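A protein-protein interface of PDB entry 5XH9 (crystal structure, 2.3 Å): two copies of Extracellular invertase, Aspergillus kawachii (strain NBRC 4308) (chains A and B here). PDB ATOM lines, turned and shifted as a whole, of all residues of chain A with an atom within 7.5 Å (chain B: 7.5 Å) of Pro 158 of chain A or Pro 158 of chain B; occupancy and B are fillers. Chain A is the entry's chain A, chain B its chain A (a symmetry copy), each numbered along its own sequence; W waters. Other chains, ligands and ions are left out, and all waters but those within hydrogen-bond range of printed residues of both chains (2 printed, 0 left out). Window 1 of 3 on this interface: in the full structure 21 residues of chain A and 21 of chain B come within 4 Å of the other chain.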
ATOM      1  N   ARG A 131      -4.547 -33.188 -15.284  1.00  0.00           N
ATOM      2  CA  ARG A 131      -3.990 -31.852 -15.495  1.00  0.00           C
ATOM      3  C   ARG A 131      -2.983 -31.500 -14.389  1.00  0.00           C
ATOM      4  O   ARG A 131      -3.254 -31.722 -13.224  1.00  0.00           O
ATOM      5  CB  ARG A 131      -5.149 -30.842 -15.498  1.00  0.00           C
ATOM      6  CG  ARG A 131      -4.742 -29.391 -15.757  1.00  0.00           C
ATOM      7  CD  ARG A 131      -4.560 -29.125 -17.237  1.00  0.00           C
ATOM      8  NE  ARG A 131      -4.248 -27.722 -17.508  1.00  0.00           N
ATOM      9  CZ  ARG A 131      -5.137 -26.725 -17.518  1.00  0.00           C
ATOM     10  NH1 ARG A 131      -6.408 -26.942 -17.240  1.00  0.00           N
ATOM     11  NH2 ARG A 131      -4.749 -25.494 -17.803  1.00  0.00           N
ATOM     12  N   GLY A 132      -1.817 -30.986 -14.757  1.00  0.00           N
ATOM     13  CA  GLY A 132      -0.814 -30.602 -13.760  1.00  0.00           C
ATOM     14  C   GLY A 132      -0.050 -31.708 -13.048  1.00  0.00           C
ATOM     15  O   GLY A 132       0.741 -31.442 -12.126  1.00  0.00           O
ATOM     16  N   SER A 133      -0.243 -32.950 -13.472  1.00  0.00           N
ATOM     17  CA  SER A 133       0.426 -34.066 -12.828  1.00  0.00           C
ATOM     18  C   SER A 133       1.933 -34.003 -13.043  1.00  0.00           C
ATOM     19  O   SER A 133       2.687 -34.431 -12.162  1.00  0.00           O
ATOM     20  CB  SER A 133      -0.116 -35.398 -13.346  1.00  0.00           C
ATOM     21  OG  SER A 133      -0.007 -35.451 -14.736  1.00  0.00           O
ATOM     22  N   GLU A 134       2.362 -33.489 -14.211  1.00  0.00           N
ATOM     23  CA  GLU A 134       3.789 -33.343 -14.539  1.00  0.00           C
ATOM     24  C   GLU A 134       4.141 -31.905 -14.942  1.00  0.00           C
ATOM     25  O   GLU A 134       3.533 -31.317 -15.836  1.00  0.00           O
ATOM     26  CB  GLU A 134       4.211 -34.304 -15.647  1.00  0.00           C
ATOM     27  CG  GLU A 134       3.932 -35.781 -15.386  1.00  0.00           C
ATOM     28  CD  GLU A 134       4.034 -36.650 -16.640  1.00  0.00           C
ATOM     29  OE1 GLU A 134       3.401 -36.307 -17.672  1.00  0.00           O
ATOM     30  OE2 GLU A 134       4.750 -37.675 -16.601  1.00  0.00           O
ATOM     31  N   THR A 135       5.124 -31.341 -14.254  1.00  0.00           N
ATOM     32  CA  THR A 135       5.618 -30.010 -14.542  1.00  0.00           C
ATOM     33  C   THR A 135       7.121 -30.115 -14.591  1.00  0.00           C
ATOM     34  O   THR A 135       7.683 -31.126 -14.178  1.00  0.00           O
ATOM     35  CB  THR A 135       5.225 -29.003 -13.446  1.00  0.00           C
ATOM     36  OG1 THR A 135       5.771 -29.418 -12.196  1.00  0.00           O
ATOM     37  CG2 THR A 135       3.698 -28.886 -13.316  1.00  0.00           C
ATOM     38  N   GLN A 136       7.780 -29.069 -15.071  1.00  0.00           N
ATOM     39  CA  GLN A 136       9.231 -29.065 -15.120  1.00  0.00           C
ATOM     40  C   GLN A 136       9.768 -27.957 -14.212  1.00  0.00           C
ATOM     41  O   GLN A 136       9.394 -26.793 -14.361  1.00  0.00           O
ATOM     42  CB  GLN A 136       9.742 -28.978 -16.569  1.00  0.00           C
ATOM     43  CG  GLN A 136       8.850 -29.651 -17.624  1.00  0.00           C
ATOM     44  CD  GLN A 136       8.542 -31.118 -17.373  1.00  0.00           C
ATOM     45  OE1 GLN A 136       9.386 -31.864 -16.860  1.00  0.00           O
ATOM     46  NE2 GLN A 136       7.319 -31.557 -17.764  1.00  0.00           N
ATOM     47  N   SER A 137      10.633 -28.352 -13.267  1.00  0.00           N
ATOM     48  CA  SER A 137      11.133 -27.502 -12.194  1.00  0.00           C
ATOM     49  C   SER A 137      12.658 -27.457 -12.189  1.00  0.00           C
ATOM     50  O   SER A 137      13.328 -28.345 -12.756  1.00  0.00           O
ATOM     51  CB  SER A 137      10.624 -28.008 -10.826  1.00  0.00           C
ATOM     52  OG  SER A 137       9.230 -27.754 -10.662  1.00  0.00           O
ATOM     53  N   GLY A 154       7.729 -21.910  -8.173  1.00  0.00           N
ATOM     54  CA  GLY A 154       6.993 -22.887  -8.930  1.00  0.00           C
ATOM     55  C   GLY A 154       7.753 -23.381 -10.144  1.00  0.00           C
ATOM     56  O   GLY A 154       8.858 -22.918 -10.431  1.00  0.00           O
ATOM     57  N   PRO A 155       7.153 -24.325 -10.873  1.00  0.00           N
ATOM     58  CA  PRO A 155       7.830 -24.897 -12.041  1.00  0.00           C
ATOM     59  C   PRO A 155       8.069 -23.862 -13.126  1.00  0.00           C
ATOM     60  O   PRO A 155       7.308 -22.912 -13.229  1.00  0.00           O
ATOM     61  CB  PRO A 155       6.842 -25.951 -12.542  1.00  0.00           C
ATOM     62  CG  PRO A 155       5.530 -25.469 -12.053  1.00  0.00           C
ATOM     63  CD  PRO A 155       5.789 -24.847 -10.720  1.00  0.00           C
ATOM     64  N   VAL A 156       9.121 -24.058 -13.916  1.00  0.00           N
ATOM     65  CA  VAL A 156       9.453 -23.132 -15.012  1.00  0.00           C
ATOM     66  C   VAL A 156       8.710 -23.482 -16.301  1.00  0.00           C
ATOM     67  O   VAL A 156       8.569 -22.635 -17.202  1.00  0.00           O
ATOM     68  CB  VAL A 156      10.971 -23.048 -15.259  1.00  0.00           C
ATOM     69  CG1 VAL A 156      11.650 -22.373 -14.066  1.00  0.00           C
ATOM     70  CG2 VAL A 156      11.575 -24.424 -15.559  1.00  0.00           C
ATOM     71  N   ILE A 157       8.255 -24.728 -16.394  1.00  0.00           N
ATOM     72  CA  ILE A 157       7.312 -25.127 -17.429  1.00  0.00           C
ATOM     73  C   ILE A 157       6.135 -25.792 -16.711  1.00  0.00           C
ATOM     74  O   ILE A 157       6.175 -26.998 -16.451  1.00  0.00           O
ATOM     75  CB  ILE A 157       7.955 -26.075 -18.479  1.00  0.00           C
ATOM     76  CG1 ILE A 157       9.148 -25.399 -19.154  1.00  0.00           C
ATOM     77  CG2 ILE A 157       6.914 -26.493 -19.513  1.00  0.00           C
ATOM     78  CD1 ILE A 157      10.053 -26.348 -19.902  1.00  0.00           C
ATOM     79  N   PRO A 158       5.077 -25.013 -16.379  1.00  0.00           N
ATOM     80  CA  PRO A 158       3.943 -25.565 -15.605  1.00  0.00           C
ATOM     81  C   PRO A 158       2.992 -26.541 -16.318  1.00  0.00           C
ATOM     82  O   PRO A 158       2.038 -27.017 -15.708  1.00  0.00           O
ATOM     83  CB  PRO A 158       3.148 -24.317 -15.194  1.00  0.00           C
ATOM     84  CG  PRO A 158       3.970 -23.131 -15.590  1.00  0.00           C
ATOM     85  CD  PRO A 158       4.897 -23.575 -16.664  1.00  0.00           C
ATOM     86  N   GLY A 159       3.211 -26.808 -17.592  1.00  0.00           N
ATOM     87  CA  GLY A 159       2.361 -27.733 -18.317  1.00  0.00           C
ATOM     88  C   GLY A 159       2.543 -27.686 -19.813  1.00  0.00           C
ATOM     89  O   GLY A 159       3.330 -26.878 -20.340  1.00  0.00           O
ATOM     90  N   PRO A 160       1.842 -28.570 -20.519  1.00  0.00           N
ATOM     91  CA  PRO A 160       1.919 -28.566 -21.971  1.00  0.00           C
ATOM     92  C   PRO A 160       1.229 -27.341 -22.536  1.00  0.00           C
ATOM     93  O   PRO A 160       0.534 -26.654 -21.798  1.00  0.00           O
ATOM     94  CB  PRO A 160       1.139 -29.821 -22.373  1.00  0.00           C
ATOM     95  CG  PRO A 160       0.220 -30.080 -21.230  1.00  0.00           C
ATOM     96  CD  PRO A 160       0.926 -29.600 -20.004  1.00  0.00           C
ATOM     97  N   PHE A 169       4.133 -35.985 -20.363  1.00  0.00           N
ATOM     98  CA  PHE A 169       4.839 -34.716 -20.496  1.00  0.00           C
ATOM     99  C   PHE A 169       6.015 -34.643 -19.498  1.00  0.00           C
ATOM    100  O   PHE A 169       5.950 -33.960 -18.482  1.00  0.00           O
ATOM    101  CB  PHE A 169       3.841 -33.587 -20.283  1.00  0.00           C
ATOM    102  CG  PHE A 169       4.367 -32.228 -20.627  1.00  0.00           C
ATOM    103  CD1 PHE A 169       4.576 -31.868 -21.946  1.00  0.00           C
ATOM    104  CD2 PHE A 169       4.582 -31.283 -19.626  1.00  0.00           C
ATOM    105  CE1 PHE A 169       5.034 -30.592 -22.262  1.00  0.00           C
ATOM    106  CE2 PHE A 169       5.044 -30.016 -19.925  1.00  0.00           C
ATOM    107  CZ  PHE A 169       5.276 -29.674 -21.242  1.00  0.00           C
ATOM    108  N   GLN A 217      14.339 -19.334 -16.827  1.00  0.00           N
ATOM    109  CA  GLN A 217      13.060 -19.168 -16.157  1.00  0.00           C
ATOM    110  C   GLN A 217      11.933 -19.456 -17.150  1.00  0.00           C
ATOM    111  O   GLN A 217      10.934 -20.079 -16.799  1.00  0.00           O
ATOM    112  CB  GLN A 217      12.993 -17.721 -15.615  1.00  0.00           C
ATOM    113  CG  GLN A 217      11.829 -17.371 -14.696  1.00  0.00           C
ATOM    114  CD  GLN A 217      11.793 -18.210 -13.422  1.00  0.00           C
ATOM    115  OE1 GLN A 217      12.829 -18.466 -12.772  1.00  0.00           O
ATOM    116  NE2 GLN A 217      10.601 -18.681 -13.084  1.00  0.00           N
ATOM    117  N   TYR A 218      12.092 -19.007 -18.396  1.00  0.00           N
ATOM    118  CA  TYR A 218      11.055 -19.165 -19.399  1.00  0.00           C
ATOM    119  C   TYR A 218      11.574 -19.972 -20.579  1.00  0.00           C
ATOM    120  O   TYR A 218      12.711 -19.786 -21.017  1.00  0.00           O
ATOM    121  CB  TYR A 218      10.528 -17.784 -19.838  1.00  0.00           C
ATOM    122  CG  TYR A 218       9.869 -17.033 -18.689  1.00  0.00           C
ATOM    123  CD1 TYR A 218       8.616 -17.437 -18.211  1.00  0.00           C
ATOM    124  CD2 TYR A 218      10.488 -15.924 -18.070  1.00  0.00           C
ATOM    125  CE1 TYR A 218       7.995 -16.780 -17.157  1.00  0.00           C
ATOM    126  CE2 TYR A 218       9.868 -15.261 -17.002  1.00  0.00           C
ATOM    127  CZ  TYR A 218       8.617 -15.711 -16.549  1.00  0.00           C
ATOM    128  OH  TYR A 218       7.957 -15.127 -15.493  1.00  0.00           O
ATOM    129  N   ARG B 131       7.536 -16.870  -9.166  1.00  0.00           N
ATOM    130  CA  ARG B 131       6.883 -17.667 -10.204  1.00  0.00           C
ATOM    131  C   ARG B 131       6.009 -18.765  -9.581  1.00  0.00           C
ATOM    132  O   ARG B 131       6.440 -19.443  -8.666  1.00  0.00           O
ATOM    133  CB  ARG B 131       7.974 -18.294 -11.088  1.00  0.00           C
ATOM    134  CG  ARG B 131       7.456 -19.126 -12.262  1.00  0.00           C
ATOM    135  CD  ARG B 131       7.070 -18.247 -13.433  1.00  0.00           C
ATOM    136  NE  ARG B 131       6.648 -19.032 -14.592  1.00  0.00           N
ATOM    137  CZ  ARG B 131       7.471 -19.660 -15.437  1.00  0.00           C
ATOM    138  NH1 ARG B 131       8.778 -19.641 -15.255  1.00  0.00           N
ATOM    139  NH2 ARG B 131       6.982 -20.321 -16.471  1.00  0.00           N
ATOM    140  N   GLY B 132       4.779 -18.917 -10.052  1.00  0.00           N
ATOM    141  CA  GLY B 132       3.892 -19.960  -9.525  1.00  0.00           C
ATOM    142  C   GLY B 132       3.290 -19.757  -8.143  1.00  0.00           C
ATOM    143  O   GLY B 132       2.611 -20.652  -7.610  1.00  0.00           O
ATOM    144  N   SER B 133       3.495 -18.586  -7.556  1.00  0.00           N
ATOM    145  CA  SER B 133       2.979 -18.324  -6.225  1.00  0.00           C
ATOM    146  C   SER B 133       1.455 -18.295  -6.222  1.00  0.00           C
ATOM    147  O   SER B 133       0.846 -18.681  -5.218  1.00  0.00           O
ATOM    148  CB  SER B 133       3.522 -17.002  -5.681  1.00  0.00           C
ATOM    149  OG  SER B 133       3.238 -15.965  -6.569  1.00  0.00           O
ATOM    150  N   GLU B 134       0.851 -17.826  -7.329  1.00  0.00           N
ATOM    151  CA  GLU B 134      -0.612 -17.768  -7.473  1.00  0.00           C
ATOM    152  C   GLU B 134      -1.093 -18.485  -8.743  1.00  0.00           C
ATOM    153  O   GLU B 134      -0.639 -18.206  -9.852  1.00  0.00           O
ATOM    154  CB  GLU B 134      -1.120 -16.329  -7.473  1.00  0.00           C
ATOM    155  CG  GLU B 134      -0.727 -15.488  -6.262  1.00  0.00           C
ATOM    156  CD  GLU B 134      -0.942 -13.988  -6.469  1.00  0.00           C
ATOM    157  OE1 GLU B 134      -0.467 -13.441  -7.498  1.00  0.00           O
ATOM    158  OE2 GLU B 134      -1.588 -13.351  -5.607  1.00  0.00           O
ATOM    159  N   THR B 135      -2.009 -19.425  -8.558  1.00  0.00           N
ATOM    160  CA  THR B 135      -2.609 -20.159  -9.654  1.00  0.00           C
ATOM    161  C   THR B 135      -4.098 -20.134  -9.417  1.00  0.00           C
ATOM    162  O   THR B 135      -4.545 -19.770  -8.332  1.00  0.00           O
ATOM    163  CB  THR B 135      -2.135 -21.622  -9.692  1.00  0.00           C
ATOM    164  OG1 THR B 135      -2.492 -22.274  -8.474  1.00  0.00           O
ATOM    165  CG2 THR B 135      -0.613 -21.712  -9.885  1.00  0.00           C
ATOM    166  N   GLN B 136      -4.871 -20.542 -10.415  1.00  0.00           N
ATOM    167  CA  GLN B 136      -6.314 -20.590 -10.264  1.00  0.00           C
ATOM    168  C   GLN B 136      -6.790 -22.039 -10.382  1.00  0.00           C
ATOM    169  O   GLN B 136      -6.504 -22.710 -11.374  1.00  0.00           O
ATOM    170  CB  GLN B 136      -7.012 -19.629 -11.242  1.00  0.00           C
ATOM    171  CG  GLN B 136      -6.227 -18.353 -11.584  1.00  0.00           C
ATOM    172  CD  GLN B 136      -5.808 -17.509 -10.390  1.00  0.00           C
ATOM    173  OE1 GLN B 136      -6.536 -17.416  -9.394  1.00  0.00           O
ATOM    174  NE2 GLN B 136      -4.623 -16.856 -10.495  1.00  0.00           N
ATOM    175  N   SER B 137      -7.503 -22.501  -9.344  1.00  0.00           N
ATOM    176  CA  SER B 137      -7.907 -23.890  -9.168  1.00  0.00           C
ATOM    177  C   SER B 137      -9.418 -24.010  -9.001  1.00  0.00           C
ATOM    178  O   SER B 137     -10.105 -23.026  -8.655  1.00  0.00           O
ATOM    179  CB  SER B 137      -7.198 -24.505  -7.941  1.00  0.00           C
ATOM    180  OG  SER B 137      -5.811 -24.720  -8.194  1.00  0.00           O
ATOM    181  N   GLY B 154      -4.329 -30.455 -10.936  1.00  0.00           N
ATOM    182  CA  GLY B 154      -3.644 -29.195 -10.835  1.00  0.00           C
ATOM    183  C   GLY B 154      -4.525 -28.019 -11.202  1.00  0.00           C
ATOM    184  O   GLY B 154      -5.682 -28.190 -11.589  1.00  0.00           O
ATOM    185  N   PRO B 155      -3.973 -26.808 -11.089  1.00  0.00           N
ATOM    186  CA  PRO B 155      -4.761 -25.607 -11.378  1.00  0.00           C
ATOM    187  C   PRO B 155      -5.196 -25.545 -12.833  1.00  0.00           C
ATOM    188  O   PRO B 155      -4.509 -26.081 -13.688  1.00  0.00           O
ATOM    189  CB  PRO B 155      -3.789 -24.464 -11.082  1.00  0.00           C
ATOM    190  CG  PRO B 155      -2.454 -25.077 -11.269  1.00  0.00           C
ATOM    191  CD  PRO B 155      -2.573 -26.484 -10.783  1.00  0.00           C
ATOM    192  N   VAL B 156      -6.329 -24.896 -13.089  1.00  0.00           N
ATOM    193  CA  VAL B 156      -6.850 -24.758 -14.460  1.00  0.00           C
ATOM    194  C   VAL B 156      -6.262 -23.542 -15.175  1.00  0.00           C
ATOM    195  O   VAL B 156      -6.286 -23.463 -16.416  1.00  0.00           O
ATOM    196  CB  VAL B 156      -8.390 -24.721 -14.491  1.00  0.00           C
ATOM    197  CG1 VAL B 156      -8.945 -26.087 -14.085  1.00  0.00           C
ATOM    198  CG2 VAL B 156      -8.950 -23.592 -13.620  1.00  0.00           C
ATOM    199  N   ILE B 157      -5.753 -22.593 -14.393  1.00  0.00           N
ATOM    200  CA  ILE B 157      -4.931 -21.517 -14.927  1.00  0.00           C
ATOM    201  C   ILE B 157      -3.637 -21.514 -14.111  1.00  0.00           C
ATOM    202  O   ILE B 157      -3.576 -20.876 -13.057  1.00  0.00           O
ATOM    203  CB  ILE B 157      -5.651 -20.140 -14.868  1.00  0.00           C
ATOM    204  CG1 ILE B 157      -6.956 -20.182 -15.662  1.00  0.00           C
ATOM    205  CG2 ILE B 157      -4.730 -19.046 -15.400  1.00  0.00           C
ATOM    206  CD1 ILE B 157      -7.897 -19.039 -15.364  1.00  0.00           C
ATOM    207  N   PRO B 158      -2.589 -22.231 -14.588  1.00  0.00           N
ATOM    208  CA  PRO B 158      -1.336 -22.349 -13.810  1.00  0.00           C
ATOM    209  C   PRO B 158      -0.432 -21.109 -13.708  1.00  0.00           C
ATOM    210  O   PRO B 158       0.617 -21.171 -13.073  1.00  0.00           O
ATOM    211  CB  PRO B 158      -0.565 -23.460 -14.538  1.00  0.00           C
ATOM    212  CG  PRO B 158      -1.497 -24.034 -15.559  1.00  0.00           C
ATOM    213  CD  PRO B 158      -2.528 -23.003 -15.845  1.00  0.00           C
ATOM    214  N   GLY B 159      -0.798 -20.015 -14.349  1.00  0.00           N
ATOM    215  CA  GLY B 159       0.001 -18.807 -14.280  1.00  0.00           C
ATOM    216  C   GLY B 159      -0.375 -17.766 -15.304  1.00  0.00           C
ATOM    217  O   GLY B 159      -1.267 -17.983 -16.144  1.00  0.00           O
ATOM    218  N   PRO B 160       0.277 -16.607 -15.231  1.00  0.00           N
ATOM    219  CA  PRO B 160       0.013 -15.562 -16.208  1.00  0.00           C
ATOM    220  C   PRO B 160       0.556 -15.956 -17.567  1.00  0.00           C
ATOM    221  O   PRO B 160       1.301 -16.924 -17.655  1.00  0.00           O
ATOM    222  CB  PRO B 160       0.804 -14.365 -15.672  1.00  0.00           C
ATOM    223  CG  PRO B 160       1.876 -14.965 -14.828  1.00  0.00           C
ATOM    224  CD  PRO B 160       1.308 -16.221 -14.255  1.00  0.00           C
ATOM    225  N   PHE B 169      -1.557 -11.754  -9.459  1.00  0.00           N
ATOM    226  CA  PHE B 169      -2.344 -12.568 -10.377  1.00  0.00           C
ATOM    227  C   PHE B 169      -3.384 -13.407  -9.602  1.00  0.00           C
ATOM    228  O   PHE B 169      -3.226 -14.609  -9.417  1.00  0.00           O
ATOM    229  CB  PHE B 169      -1.391 -13.443 -11.180  1.00  0.00           C
ATOM    230  CG  PHE B 169      -2.033 -14.156 -12.328  1.00  0.00           C
ATOM    231  CD1 PHE B 169      -2.430 -13.460 -13.456  1.00  0.00           C
ATOM    232  CD2 PHE B 169      -2.169 -15.543 -12.308  1.00  0.00           C
ATOM    233  CE1 PHE B 169      -2.996 -14.133 -14.535  1.00  0.00           C
ATOM    234  CE2 PHE B 169      -2.735 -16.222 -13.369  1.00  0.00           C
ATOM    235  CZ  PHE B 169      -3.155 -15.516 -14.479  1.00  0.00           C
ATOM    236  N   GLN B 217     -12.134 -26.325 -17.810  1.00  0.00           N
ATOM    237  CA  GLN B 217     -10.790 -26.853 -17.641  1.00  0.00           C
ATOM    238  C   GLN B 217      -9.787 -25.873 -18.250  1.00  0.00           C
ATOM    239  O   GLN B 217      -8.718 -25.643 -17.690  1.00  0.00           O
ATOM    240  CB  GLN B 217     -10.735 -28.236 -18.331  1.00  0.00           C
ATOM    241  CG  GLN B 217      -9.483 -29.077 -18.112  1.00  0.00           C
ATOM    242  CD  GLN B 217      -9.237 -29.421 -16.647  1.00  0.00           C
ATOM    243  OE1 GLN B 217     -10.164 -29.774 -15.887  1.00  0.00           O
ATOM    244  NE2 GLN B 217      -7.986 -29.276 -16.230  1.00  0.00           N
ATOM    245  N   TYR B 218     -10.130 -25.287 -19.398  1.00  0.00           N
ATOM    246  CA  TYR B 218      -9.224 -24.395 -20.097  1.00  0.00           C
ATOM    247  C   TYR B 218      -9.845 -23.015 -20.245  1.00  0.00           C
ATOM    248  O   TYR B 218     -11.037 -22.888 -20.530  1.00  0.00           O
ATOM    249  CB  TYR B 218      -8.836 -24.996 -21.463  1.00  0.00           C
ATOM    250  CG  TYR B 218      -8.077 -26.308 -21.314  1.00  0.00           C
ATOM    251  CD1 TYR B 218      -6.752 -26.306 -20.859  1.00  0.00           C
ATOM    252  CD2 TYR B 218      -8.672 -27.553 -21.618  1.00  0.00           C
ATOM    253  CE1 TYR B 218      -6.038 -27.487 -20.701  1.00  0.00           C
ATOM    254  CE2 TYR B 218      -7.957 -28.748 -21.455  1.00  0.00           C
ATOM    255  CZ  TYR B 218      -6.635 -28.696 -20.985  1.00  0.00           C
ATOM    256  OH  TYR B 218      -5.877 -29.826 -20.777  1.00  0.00           O
HETATM  257  O   HOH W   1       4.957 -21.698 -12.127  1.00  0.00           O
HETATM  258  O   HOH W   2      -2.107 -27.582 -14.125  1.00  0.00           O
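NH2 of Arg 131 of chain A lies within hydrogen-bond range of O of Val 156 of chain B (2.9 Å).
The backbone carbonyl oxygen of Val 156 of chain A lies within hydrogen-bond range of the guanidinium group of Arg 131 of chain B (2.9 Å).
N of Gly 154 of chain A lies within hydrogen-bond range of O of Arg 131 of chain B, 2.8 Å away.
NH1 of Arg 131 of chain B lies within hydrogen-bond range of O of Gln 217 of chain A (2.7 Å).
The backbone carbonyl oxygen of Arg 131 of chain A is in hydrogen-bond range of the backbone NH of Gly 154 of chain B (2.8 Å).
The guanidinium group (NH1) of Arg 131 of chain A is in hydrogen-bond range of the backbone carbonyl oxygen (O) of Gln 217 of chain B.
N of Val 156 of chain B lies within hydrogen-bond range of O of Gln 136 of chain B.
O of Gln 136 of chain A is in hydrogen-bond range of N of Val 156 of chain A (2.8 Å).
CG of Arg 131 of chain A touches O of Pro 155 of chain B, 3.9 Å away.
Arg 131 of chain A touches Pro 158 of chain B (NH2 to CD, 3.9 Å).
CE1 of Tyr 218 of chain B touches CZ of Arg 131 of chain A (3.4 Å).
Pro 155 of chain A touches Arg 131 of chain B (O to CG, 3.9 Å).
Pro 158 of chain A touches Arg 131 of chain B.
CB of Pro 158 of chain B touches CB of Pro 158 of chain A, 3.9 Å away.
Tyr 218 of chain A touches Arg 131 of chain B.
Of the printed residues of chain B, Val 156 of chain A touches Arg 131.
Of the printed residues of chain B, Gln 217 of chain A touches Arg 131.
Of the printed residues of chain B, Tyr 218 of chain A touches Arg 131.
Ser 137 of chain B touches none of the printed residues of chain A.
Printed residues of chain A within 4 Å of Val 156 of chain B: Arg 131.
Pro 158 of chain B touches just these residues of chain A: Arg 131 and Pro 158.
Phe 169 of chain B touches none of the printed residues of chain A.
Of the printed residues of chain A, Gln 217 of chain B touches Arg 131.
The nearest residue of chain B that does not touch Pro 158 of chain A is Gly 159 of chain B (5.8 Å).
Of the 17 printed residues of chain B, 7 touch a printed residue of chain A.
Hydrophobic or aromatic side chains of chain B that line the printed part of chain A: Pro 158 and Tyr 218.
Of the 17 printed residues of chain A, 7 touch a printed residue of chain B.
Hydrophobic or aromatic side chains of chain A that line the printed part of chain B: Pro 158 and Tyr 218.
Among the printed residues, 13 pairs touch across the chains.
Among the printed residues, no Asp or Glu carboxylate lies within 4 Å of a Lys or Arg side-chain nitrogen of the other chain.
Arg 131 of chain A touches Val 156 of chain B, and with the chains exchanged Val 156 of chain A touches Arg 131 of chain B.
Arg 131 of chain A touches Gln 217 of chain B, and with the chains exchanged Gln 217 of chain A touches Arg 131 of chain B.
Arg 131 of chain A touches Tyr 218 of chain B, and with the chains exchanged Tyr 218 of chain A touches Arg 131 of chain B.
Pro 158 of chain A touches its own counterpart, Pro 158 of chain B.
Positions printed for both chains: 131, 132, 133, 134, 135, 136, 137, 154, 155, 156, 157, 158, 159, 160, 169, 217 and 218.
Of the 13 pairs that touch across the chains among the printed residues, 13 have their exchanged pair printed and touching as well.
Water W1 bridges the backbone carbonyl oxygen (O) of Pro 155 of chain A and the backbone NH (N) of Gly 132 of chain B.
Water W2 bridges O of Pro 155 of chain B (2.9 Å) and N of Gly 132 of chain A (3.5 Å).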
